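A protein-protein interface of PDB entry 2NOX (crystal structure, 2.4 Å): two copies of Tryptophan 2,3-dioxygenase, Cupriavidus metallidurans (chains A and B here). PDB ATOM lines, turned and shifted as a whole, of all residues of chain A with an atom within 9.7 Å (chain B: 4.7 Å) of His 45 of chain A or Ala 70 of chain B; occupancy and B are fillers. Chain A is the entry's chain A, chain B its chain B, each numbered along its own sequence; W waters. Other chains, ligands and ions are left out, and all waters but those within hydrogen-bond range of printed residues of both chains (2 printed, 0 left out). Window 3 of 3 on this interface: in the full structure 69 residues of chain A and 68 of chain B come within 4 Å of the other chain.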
ATOM      1  N   PRO A  40      32.385 -14.418  10.367  1.00  0.00           N
ATOM      2  CA  PRO A  40      31.057 -14.039  10.857  1.00  0.00           C
ATOM      3  C   PRO A  40      29.990 -14.987  10.331  1.00  0.00           C
ATOM      4  O   PRO A  40      30.020 -15.382   9.182  1.00  0.00           O
ATOM      5  CB  PRO A  40      30.842 -12.621  10.301  1.00  0.00           C
ATOM      6  CG  PRO A  40      31.846 -12.441   9.252  1.00  0.00           C
ATOM      7  CD  PRO A  40      32.995 -13.369   9.537  1.00  0.00           C
ATOM      8  N   LEU A  41      29.056 -15.313  11.194  1.00  0.00           N
ATOM      9  CA  LEU A  41      28.065 -16.316  10.962  1.00  0.00           C
ATOM     10  C   LEU A  41      26.737 -15.665  10.608  1.00  0.00           C
ATOM     11  O   LEU A  41      25.940 -16.267   9.916  1.00  0.00           O
ATOM     12  CB  LEU A  41      27.903 -17.148  12.244  1.00  0.00           C
ATOM     13  CG  LEU A  41      28.595 -18.519  12.306  1.00  0.00           C
ATOM     14  CD1 LEU A  41      29.869 -18.567  11.544  1.00  0.00           C
ATOM     15  CD2 LEU A  41      28.816 -18.907  13.734  1.00  0.00           C
ATOM     16  N   SER A  42      26.514 -14.437  11.079  1.00  0.00           N
ATOM     17  CA  SER A  42      25.277 -13.696  10.814  1.00  0.00           C
ATOM     18  C   SER A  42      25.441 -12.772   9.638  1.00  0.00           C
ATOM     19  O   SER A  42      26.553 -12.477   9.220  1.00  0.00           O
ATOM     20  CB  SER A  42      24.882 -12.843  12.014  1.00  0.00           C
ATOM     21  OG  SER A  42      25.503 -11.565  11.947  1.00  0.00           O
ATOM     22  N   PRO A  43      24.313 -12.280   9.107  1.00  0.00           N
ATOM     23  CA  PRO A  43      24.325 -11.262   8.055  1.00  0.00           C
ATOM     24  C   PRO A  43      24.638  -9.846   8.574  1.00  0.00           C
ATOM     25  O   PRO A  43      24.926  -8.962   7.771  1.00  0.00           O
ATOM     26  CB  PRO A  43      22.927 -11.342   7.459  1.00  0.00           C
ATOM     27  CG  PRO A  43      22.107 -12.167   8.400  1.00  0.00           C
ATOM     28  CD  PRO A  43      22.957 -12.685   9.495  1.00  0.00           C
ATOM     29  N   ASP A  44      24.668  -9.672   9.900  1.00  0.00           N
ATOM     30  CA  ASP A  44      24.867  -8.353  10.536  1.00  0.00           C
ATOM     31  C   ASP A  44      26.263  -7.727  10.410  1.00  0.00           C
ATOM     32  O   ASP A  44      27.302  -8.380  10.588  1.00  0.00           O
ATOM     33  CB  ASP A  44      24.419  -8.392  12.009  1.00  0.00           C
ATOM     34  CG  ASP A  44      24.157  -7.011  12.579  1.00  0.00           C
ATOM     35  OD1 ASP A  44      25.128  -6.326  12.947  1.00  0.00           O
ATOM     36  OD2 ASP A  44      22.983  -6.584  12.644  1.00  0.00           O
ATOM     37  N   HIS A  45      26.261  -6.439  10.100  1.00  0.00           N
ATOM     38  CA  HIS A  45      27.459  -5.617   9.930  1.00  0.00           C
ATOM     39  C   HIS A  45      28.357  -5.501  11.181  1.00  0.00           C
ATOM     40  O   HIS A  45      29.561  -5.184  11.112  1.00  0.00           O
ATOM     41  CB  HIS A  45      26.983  -4.229   9.576  1.00  0.00           C
ATOM     42  CG  HIS A  45      28.050  -3.193   9.674  1.00  0.00           C
ATOM     43  ND1 HIS A  45      29.008  -3.030   8.699  1.00  0.00           N
ATOM     44  CD2 HIS A  45      28.319  -2.274  10.632  1.00  0.00           C
ATOM     45  CE1 HIS A  45      29.819  -2.045   9.050  1.00  0.00           C
ATOM     46  NE2 HIS A  45      29.429  -1.580  10.224  1.00  0.00           N
ATOM     47  N   ASN A  46      27.730  -5.701  12.327  1.00  0.00           N
ATOM     48  CA  ASN A  46      28.357  -5.438  13.589  1.00  0.00           C
ATOM     49  C   ASN A  46      29.043  -6.676  14.144  1.00  0.00           C
ATOM     50  O   ASN A  46      29.591  -6.634  15.244  1.00  0.00           O
ATOM     51  CB  ASN A  46      27.304  -4.945  14.571  1.00  0.00           C
ATOM     52  CG  ASN A  46      26.673  -3.631  14.129  1.00  0.00           C
ATOM     53  OD1 ASN A  46      27.219  -2.543  14.402  1.00  0.00           O
ATOM     54  ND2 ASN A  46      25.534  -3.721  13.411  1.00  0.00           N
ATOM     55  N   GLU A  47      29.010  -7.773  13.387  1.00  0.00           N
ATOM     56  CA  GLU A  47      29.580  -9.013  13.880  1.00  0.00           C
ATOM     57  C   GLU A  47      31.098  -8.995  13.761  1.00  0.00           C
ATOM     58  O   GLU A  47      31.795  -9.555  14.642  1.00  0.00           O
ATOM     59  CB  GLU A  47      28.966 -10.261  13.226  1.00  0.00           C
ATOM     60  CG  GLU A  47      29.639 -11.569  13.711  1.00  0.00           C
ATOM     61  CD  GLU A  47      28.878 -12.814  13.305  1.00  0.00           C
ATOM     62  OE1 GLU A  47      27.898 -12.698  12.546  1.00  0.00           O
ATOM     63  OE2 GLU A  47      29.243 -13.914  13.761  1.00  0.00           O
ATOM     64  N   MET A  48      31.630  -8.352  12.712  1.00  0.00           N
ATOM     65  CA  MET A  48      33.095  -8.210  12.631  1.00  0.00           C
ATOM     66  C   MET A  48      33.659  -7.574  13.937  1.00  0.00           C
ATOM     67  O   MET A  48      34.678  -8.007  14.461  1.00  0.00           O
ATOM     68  CB  MET A  48      33.511  -7.418  11.383  1.00  0.00           C
ATOM     69  CG  MET A  48      34.979  -7.553  10.955  1.00  0.00           C
ATOM     70  SD  MET A  48      35.508  -9.240  10.461  1.00  0.00           S
ATOM     71  CE  MET A  48      34.658  -9.396   8.888  1.00  0.00           C
ATOM     72  N   LEU A  49      32.982  -6.558  14.468  1.00  0.00           N
ATOM     73  CA  LEU A  49      33.404  -5.964  15.732  1.00  0.00           C
ATOM     74  C   LEU A  49      33.389  -7.014  16.849  1.00  0.00           C
ATOM     75  O   LEU A  49      34.322  -7.125  17.627  1.00  0.00           O
ATOM     76  CB  LEU A  49      32.504  -4.771  16.118  1.00  0.00           C
ATOM     77  CG  LEU A  49      32.707  -4.297  17.552  1.00  0.00           C
ATOM     78  CD1 LEU A  49      34.119  -3.764  17.812  1.00  0.00           C
ATOM     79  CD2 LEU A  49      31.704  -3.295  17.922  1.00  0.00           C
ATOM     80  N   PHE A  50      32.320  -7.783  16.939  1.00  0.00           N
ATOM     81  CA  PHE A  50      32.242  -8.788  18.001  1.00  0.00           C
ATOM     82  C   PHE A  50      33.430  -9.769  17.932  1.00  0.00           C
ATOM     83  O   PHE A  50      33.977 -10.189  18.952  1.00  0.00           O
ATOM     84  CB  PHE A  50      30.910  -9.533  17.894  1.00  0.00           C
ATOM     85  CG  PHE A  50      30.619 -10.438  19.053  1.00  0.00           C
ATOM     86  CD1 PHE A  50      30.259  -9.918  20.273  1.00  0.00           C
ATOM     87  CD2 PHE A  50      30.717 -11.821  18.918  1.00  0.00           C
ATOM     88  CE1 PHE A  50      29.978 -10.765  21.356  1.00  0.00           C
ATOM     89  CE2 PHE A  50      30.448 -12.664  19.974  1.00  0.00           C
ATOM     90  CZ  PHE A  50      30.071 -12.137  21.196  1.00  0.00           C
ATOM     91  N   ILE A  51      33.832 -10.111  16.716  1.00  0.00           N
ATOM     92  CA  ILE A  51      34.898 -11.074  16.514  1.00  0.00           C
ATOM     93  C   ILE A  51      36.294 -10.464  16.780  1.00  0.00           C
ATOM     94  O   ILE A  51      37.103 -11.006  17.559  1.00  0.00           O
ATOM     95  CB  ILE A  51      34.813 -11.649  15.095  1.00  0.00           C
ATOM     96  CG1 ILE A  51      33.602 -12.597  15.001  1.00  0.00           C
ATOM     97  CG2 ILE A  51      36.063 -12.361  14.760  1.00  0.00           C
ATOM     98  CD1 ILE A  51      33.240 -12.955  13.589  1.00  0.00           C
ATOM     99  N   VAL A  52      36.557  -9.318  16.156  1.00  0.00           N
ATOM    100  CA  VAL A  52      37.859  -8.689  16.275  1.00  0.00           C
ATOM    101  C   VAL A  52      38.118  -8.230  17.705  1.00  0.00           C
ATOM    102  O   VAL A  52      39.233  -8.392  18.228  1.00  0.00           O
ATOM    103  CB  VAL A  52      38.000  -7.556  15.285  1.00  0.00           C
ATOM    104  CG1 VAL A  52      39.179  -6.645  15.663  1.00  0.00           C
ATOM    105  CG2 VAL A  52      38.103  -8.130  13.833  1.00  0.00           C
ATOM    106  N   THR A 106      30.163   0.658  21.547  1.00  0.00           N
ATOM    107  CA  THR A 106      29.467   1.231  20.409  1.00  0.00           C
ATOM    108  C   THR A 106      28.481   0.220  19.788  1.00  0.00           C
ATOM    109  O   THR A 106      27.801   0.521  18.794  1.00  0.00           O
ATOM    110  CB  THR A 106      30.443   1.736  19.303  1.00  0.00           C
ATOM    111  OG1 THR A 106      31.094   0.629  18.670  1.00  0.00           O
ATOM    112  CG2 THR A 106      31.472   2.731  19.854  1.00  0.00           C
ATOM    113  N   MET A 107      28.418  -0.978  20.370  1.00  0.00           N
ATOM    114  CA  MET A 107      27.422  -1.954  19.966  1.00  0.00           C
ATOM    115  C   MET A 107      26.090  -1.770  20.733  1.00  0.00           C
ATOM    116  O   MET A 107      26.077  -1.720  21.973  1.00  0.00           O
ATOM    117  CB  MET A 107      27.929  -3.377  20.181  1.00  0.00           C
ATOM    118  CG  MET A 107      27.002  -4.396  19.551  1.00  0.00           C
ATOM    119  SD  MET A 107      27.682  -6.016  19.600  1.00  0.00           S
ATOM    120  CE  MET A 107      28.283  -6.052  17.957  1.00  0.00           C
ATOM    121  N   PRO A 110      19.970  -3.881  19.700  1.00  0.00           N
ATOM    122  CA  PRO A 110      19.453  -4.494  18.460  1.00  0.00           C
ATOM    123  C   PRO A 110      20.561  -5.084  17.555  1.00  0.00           C
ATOM    124  O   PRO A 110      20.353  -6.139  16.951  1.00  0.00           O
ATOM    125  CB  PRO A 110      18.668  -3.354  17.776  1.00  0.00           C
ATOM    126  CG  PRO A 110      19.038  -2.089  18.516  1.00  0.00           C
ATOM    127  CD  PRO A 110      19.572  -2.458  19.846  1.00  0.00           C
ATOM    128  N   GLU A 111      21.716  -4.414  17.472  1.00  0.00           N
ATOM    129  CA  GLU A 111      22.860  -4.896  16.675  1.00  0.00           C
ATOM    130  C   GLU A 111      23.282  -6.285  17.123  1.00  0.00           C
ATOM    131  O   GLU A 111      23.528  -7.168  16.306  1.00  0.00           O
ATOM    132  CB  GLU A 111      24.052  -3.931  16.767  1.00  0.00           C
ATOM    133  CG  GLU A 111      23.796  -2.606  16.042  1.00  0.00           C
ATOM    134  CD  GLU A 111      24.842  -1.511  16.274  1.00  0.00           C
ATOM    135  OE1 GLU A 111      25.830  -1.695  17.051  1.00  0.00           O
ATOM    136  OE2 GLU A 111      24.665  -0.444  15.634  1.00  0.00           O
ATOM    137  N   TYR A 112      23.364  -6.468  18.434  1.00  0.00           N
ATOM    138  CA  TYR A 112      23.769  -7.738  19.013  1.00  0.00           C
ATOM    139  C   TYR A 112      22.682  -8.770  18.900  1.00  0.00           C
ATOM    140  O   TYR A 112      22.962  -9.929  18.616  1.00  0.00           O
ATOM    141  CB  TYR A 112      24.187  -7.606  20.484  1.00  0.00           C
ATOM    142  CG  TYR A 112      24.699  -8.907  21.081  1.00  0.00           C
ATOM    143  CD1 TYR A 112      23.992  -9.560  22.101  1.00  0.00           C
ATOM    144  CD2 TYR A 112      25.896  -9.493  20.626  1.00  0.00           C
ATOM    145  CE1 TYR A 112      24.443 -10.751  22.660  1.00  0.00           C
ATOM    146  CE2 TYR A 112      26.379 -10.706  21.180  1.00  0.00           C
ATOM    147  CZ  TYR A 112      25.646 -11.321  22.201  1.00  0.00           C
ATOM    148  OH  TYR A 112      26.102 -12.503  22.744  1.00  0.00           O
ATOM    149  N   ALA A 114      20.703  -9.193  16.528  1.00  0.00           N
ATOM    150  CA  ALA A 114      20.668  -9.666  15.163  1.00  0.00           C
ATOM    151  C   ALA A 114      21.655 -10.811  14.903  1.00  0.00           C
ATOM    152  O   ALA A 114      21.393 -11.686  14.074  1.00  0.00           O
ATOM    153  CB  ALA A 114      20.918  -8.504  14.205  1.00  0.00           C
ATOM    154  N   MET A 115      22.792 -10.803  15.596  1.00  0.00           N
ATOM    155  CA  MET A 115      23.796 -11.856  15.424  1.00  0.00           C
ATOM    156  C   MET A 115      23.690 -12.945  16.498  1.00  0.00           C
ATOM    157  O   MET A 115      24.234 -14.050  16.361  1.00  0.00           O
ATOM    158  CB  MET A 115      25.231 -11.282  15.350  1.00  0.00           C
ATOM    159  CG  MET A 115      25.629 -10.314  16.476  1.00  0.00           C
ATOM    160  SD  MET A 115      27.419 -10.054  16.647  1.00  0.00           S
ATOM    161  CE  MET A 115      27.857 -11.540  17.537  1.00  0.00           C
ATOM    162  N   HIS B  66      36.465  -2.399   7.369  1.00  0.00           N
ATOM    163  CA  HIS B  66      35.095  -2.880   7.374  1.00  0.00           C
ATOM    164  C   HIS B  66      34.138  -1.719   7.669  1.00  0.00           C
ATOM    165  O   HIS B  66      33.168  -1.520   6.956  1.00  0.00           O
ATOM    166  CB  HIS B  66      34.991  -4.008   8.411  1.00  0.00           C
ATOM    167  CG  HIS B  66      33.626  -4.590   8.565  1.00  0.00           C
ATOM    168  ND1 HIS B  66      33.116  -5.536   7.700  1.00  0.00           N
ATOM    169  CD2 HIS B  66      32.672  -4.378   9.500  1.00  0.00           C
ATOM    170  CE1 HIS B  66      31.901  -5.875   8.094  1.00  0.00           C
ATOM    171  NE2 HIS B  66      31.608  -5.188   9.184  1.00  0.00           N
ATOM    172  N   GLU B  67      34.432  -0.934   8.691  1.00  0.00           N
ATOM    173  CA  GLU B  67      33.583   0.197   9.055  1.00  0.00           C
ATOM    174  C   GLU B  67      33.729   1.432   8.140  1.00  0.00           C
ATOM    175  O   GLU B  67      32.764   2.153   7.870  1.00  0.00           O
ATOM    176  CB  GLU B  67      33.820   0.622  10.497  1.00  0.00           C
ATOM    177  CG  GLU B  67      33.718  -0.502  11.487  1.00  0.00           C
ATOM    178  CD  GLU B  67      32.305  -0.908  11.792  1.00  0.00           C
ATOM    179  OE1 GLU B  67      31.369  -0.099  11.519  1.00  0.00           O
ATOM    180  OE2 GLU B  67      32.153  -2.040  12.333  1.00  0.00           O
ATOM    181  N   LEU B  68      34.930   1.694   7.678  1.00  0.00           N
ATOM    182  CA  LEU B  68      35.127   2.802   6.744  1.00  0.00           C
ATOM    183  C   LEU B  68      34.386   2.580   5.442  1.00  0.00           C
ATOM    184  O   LEU B  68      33.742   3.514   4.925  1.00  0.00           O
ATOM    185  CB  LEU B  68      36.611   3.005   6.440  1.00  0.00           C
ATOM    186  CG  LEU B  68      37.319   3.643   7.630  1.00  0.00           C
ATOM    187  CD1 LEU B  68      38.818   3.554   7.436  1.00  0.00           C
ATOM    188  CD2 LEU B  68      36.841   5.109   7.785  1.00  0.00           C
ATOM    189  N   ARG B  69      34.466   1.357   4.907  1.00  0.00           N
ATOM    190  CA  ARG B  69      33.782   1.049   3.657  1.00  0.00           C
ATOM    191  C   ARG B  69      32.279   1.231   3.807  1.00  0.00           C
ATOM    192  O   ARG B  69      31.652   1.801   2.941  1.00  0.00           O
ATOM    193  CB  ARG B  69      34.111  -0.360   3.133  1.00  0.00           C
ATOM    194  CG  ARG B  69      35.565  -0.517   2.792  1.00  0.00           C
ATOM    195  CD  ARG B  69      35.945  -1.875   2.209  1.00  0.00           C
ATOM    196  NE  ARG B  69      37.169  -1.648   1.452  1.00  0.00           N
ATOM    197  CZ  ARG B  69      38.311  -2.276   1.662  1.00  0.00           C
ATOM    198  NH1 ARG B  69      38.372  -3.262   2.571  1.00  0.00           N
ATOM    199  NH2 ARG B  69      39.372  -1.931   0.929  1.00  0.00           N
ATOM    200  N   ALA B  70      31.725   0.760   4.918  1.00  0.00           N
ATOM    201  CA  ALA B  70      30.294   0.901   5.191  1.00  0.00           C
ATOM    202  C   ALA B  70      29.909   2.367   5.437  1.00  0.00           C
ATOM    203  O   ALA B  70      28.936   2.868   4.886  1.00  0.00           O
ATOM    204  CB  ALA B  70      29.884   0.031   6.347  1.00  0.00           C
ATOM    205  N   ALA B  71      30.696   3.071   6.235  1.00  0.00           N
ATOM    206  CA  ALA B  71      30.528   4.505   6.359  1.00  0.00           C
ATOM    207  C   ALA B  71      30.481   5.245   5.008  1.00  0.00           C
ATOM    208  O   ALA B  71      29.584   6.070   4.772  1.00  0.00           O
ATOM    209  CB  ALA B  71      31.612   5.072   7.228  1.00  0.00           C
ATOM    210  N   ARG B  72      31.463   4.976   4.146  1.00  0.00           N
ATOM    211  CA  ARG B  72      31.513   5.581   2.820  1.00  0.00           C
ATOM    212  C   ARG B  72      30.267   5.238   2.003  1.00  0.00           C
ATOM    213  O   ARG B  72      29.790   6.080   1.231  1.00  0.00           O
ATOM    214  CB  ARG B  72      32.748   5.127   2.055  1.00  0.00           C
ATOM    215  CG  ARG B  72      32.824   5.773   0.668  1.00  0.00           C
ATOM    216  CD  ARG B  72      34.074   5.398  -0.101  1.00  0.00           C
ATOM    217  NE  ARG B  72      34.333   3.962  -0.132  1.00  0.00           N
ATOM    218  CZ  ARG B  72      35.479   3.422  -0.553  1.00  0.00           C
ATOM    219  NH1 ARG B  72      36.447   4.202  -1.004  1.00  0.00           N
ATOM    220  NH2 ARG B  72      35.659   2.098  -0.516  1.00  0.00           N
ATOM    221  N   ASP B  73      29.745   4.012   2.168  1.00  0.00           N
ATOM    222  CA  ASP B  73      28.487   3.607   1.539  1.00  0.00           C
ATOM    223  C   ASP B  73      27.327   4.496   1.960  1.00  0.00           C
ATOM    224  O   ASP B  73      26.488   4.843   1.140  1.00  0.00           O
ATOM    225  CB  ASP B  73      28.106   2.175   1.927  1.00  0.00           C
ATOM    226  CG  ASP B  73      28.830   1.136   1.118  1.00  0.00           C
ATOM    227  OD1 ASP B  73      29.482   1.499   0.107  1.00  0.00           O
ATOM    228  OD2 ASP B  73      28.748  -0.048   1.521  1.00  0.00           O
ATOM    229  N   GLY B  74      27.256   4.808   3.254  1.00  0.00           N
ATOM    230  CA  GLY B  74      26.235   5.701   3.780  1.00  0.00           C
ATOM    231  C   GLY B  74      26.445   7.134   3.301  1.00  0.00           C
ATOM    232  O   GLY B  74      25.478   7.875   3.081  1.00  0.00           O
ATOM    233  N   MET B  86      29.217   4.730  12.568  1.00  0.00           N
ATOM    234  CA  MET B  86      30.346   3.931  12.159  1.00  0.00           C
ATOM    235  C   MET B  86      31.653   4.670  12.356  1.00  0.00           C
ATOM    236  O   MET B  86      32.668   4.107  12.803  1.00  0.00           O
ATOM    237  CB  MET B  86      30.155   3.529  10.711  1.00  0.00           C
ATOM    238  CG  MET B  86      28.880   2.706  10.532  1.00  0.00           C
ATOM    239  SD  MET B  86      28.582   2.339   8.808  1.00  0.00           S
ATOM    240  CE  MET B  86      26.867   1.888   8.865  1.00  0.00           C
ATOM    241  N   ARG B  89      32.722   4.677  15.857  1.00  0.00           N
ATOM    242  CA  ARG B  89      33.393   3.422  16.182  1.00  0.00           C
ATOM    243  C   ARG B  89      34.826   3.451  15.649  1.00  0.00           C
ATOM    244  O   ARG B  89      35.778   3.047  16.341  1.00  0.00           O
ATOM    245  CB  ARG B  89      32.598   2.229  15.606  1.00  0.00           C
ATOM    246  CG  ARG B  89      33.100   0.860  16.025  1.00  0.00           C
ATOM    247  CD  ARG B  89      32.360  -0.238  15.318  1.00  0.00           C
ATOM    248  NE  ARG B  89      31.057  -0.430  15.951  1.00  0.00           N
ATOM    249  CZ  ARG B  89      30.080  -1.207  15.489  1.00  0.00           C
ATOM    250  NH1 ARG B  89      30.216  -1.894  14.371  1.00  0.00           N
ATOM    251  NH2 ARG B  89      28.981  -1.326  16.181  1.00  0.00           N
HETATM  252  O   HOH W   1      31.578  -4.499  12.762  1.00  0.00           O
HETATM  253  O   HOH W   2      28.900   2.274  16.067  1.00  0.00           O
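NE2 of His 66 of chain B lies within hydrogen-bond range of O of His 45 of chain A. NE2 of His 45 of chain A lies within hydrogen-bond range of OE1 of Glu 67 of chain B, 2.8 Å away. NH2 of Arg 89 of chain B sits at hydrogen-bond distance from OD1 of Asn 46 of chain A, 2.8 Å away. The side-chain hydroxyl (OG1) of Thr 106 of chain A lies within hydrogen-bond range of the guanidinium group (NE) of Arg 89 of chain B, at 2.9 Å. OE1 of Glu 111 of chain A lies within salt-bridge range of NH2 of Arg 89 of chain B (3.3 Å).
ND2 of Asn 46 of chain A sits at hydrogen-bond distance from OD1 of Asp 44 of chain A (2.7 Å). OE1 of Glu 111 of chain A sits close to OD1 of Asn 46 of chain A (3.1 Å). NH1 of Arg 89 of chain B is in salt-bridge range of OE2 of Glu 67 of chain B (2.8 Å).
His 45 of chain A touches Ala 70 of chain B (CE1 to CB, 3.4 Å). Met 48 of chain A touches His 66 of chain B. Leu 49 of chain A touches Arg 89 of chain B.
Of chain B, only His 66 (2.8 Å), Glu 67 (2.8 Å) and Ala 70 (3.4 Å) come within 4 Å of His 45 of chain A. Ala 70 of chain B touches just one residue of chain A: His 45 (3.4 Å). Of chain A, only His 45 comes within 4 Å of Glu 67 of chain B. No residue of chain A comes within 4 Å of Ala 71 of chain B. No residue of chain A comes within 4 Å of Asp 73 of chain B. Of the printed residues of chain A, His 66 of chain B touches His 45 (2.8 Å) and Met 48 (3.7 Å). Printed residues of chain B within 4 Å of Glu 111 of chain A: Arg 89 (3.3 Å). Printed residues of chain B within 4 Å of Thr 106 of chain A: Arg 89 (2.9 Å). Glu 47 of chain A touches none of the printed residues of chain B. The nearest printed residue of chain A that does not touch His 66 of chain B is Asn 46 of chain A (5.0 Å).
Of the 11 printed residues of chain B, 4 touch a printed residue of chain A. Printed residues of chain B that touch a printed residue of chain A: His 66, Glu 67, Ala 70 and Arg 89. Hydrophobic or aromatic side chains of chain B that line the printed part of chain A: His 66 and Ala 70. Along chain B the printed residues that touch a printed residue of chain A span positions 66 to 89. Of the 20 printed residues of chain A, 6 touch a printed residue of chain B. Hydrophobic or aromatic side chains of chain A within 4 Å of the printed part of chain B: His 45, Met 48 and Leu 49. Along chain A the printed residues that touch a printed residue of chain B span positions 45 to 111. Among the printed residues, 8 pairs touch across the chains. Among the printed residues, Asp or Glu carboxylates within 4 Å of a Lys or Arg side-chain nitrogen of the other chain: Glu 111 of chain A with Arg 89 of chain B (3.3 Å).
No position is printed for both chains.
Water W1 lies within hydrogen-bond range of the side-chain carboxylate (OE2) of Glu 67 of chain B (2.6 Å), the backbone carbonyl oxygen (O) of His 45 of chain A (2.7 Å), the backbone NH (N) of Leu 49 of chain A (3.0 Å) and the guanidinium group (NH1) of Arg 89 of chain B (3.4 Å). Water W2 lies within hydrogen-bond range of O of Thr 106 of chain A (3.4 Å) and NE of Arg 89 of chain B (3.5 Å).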
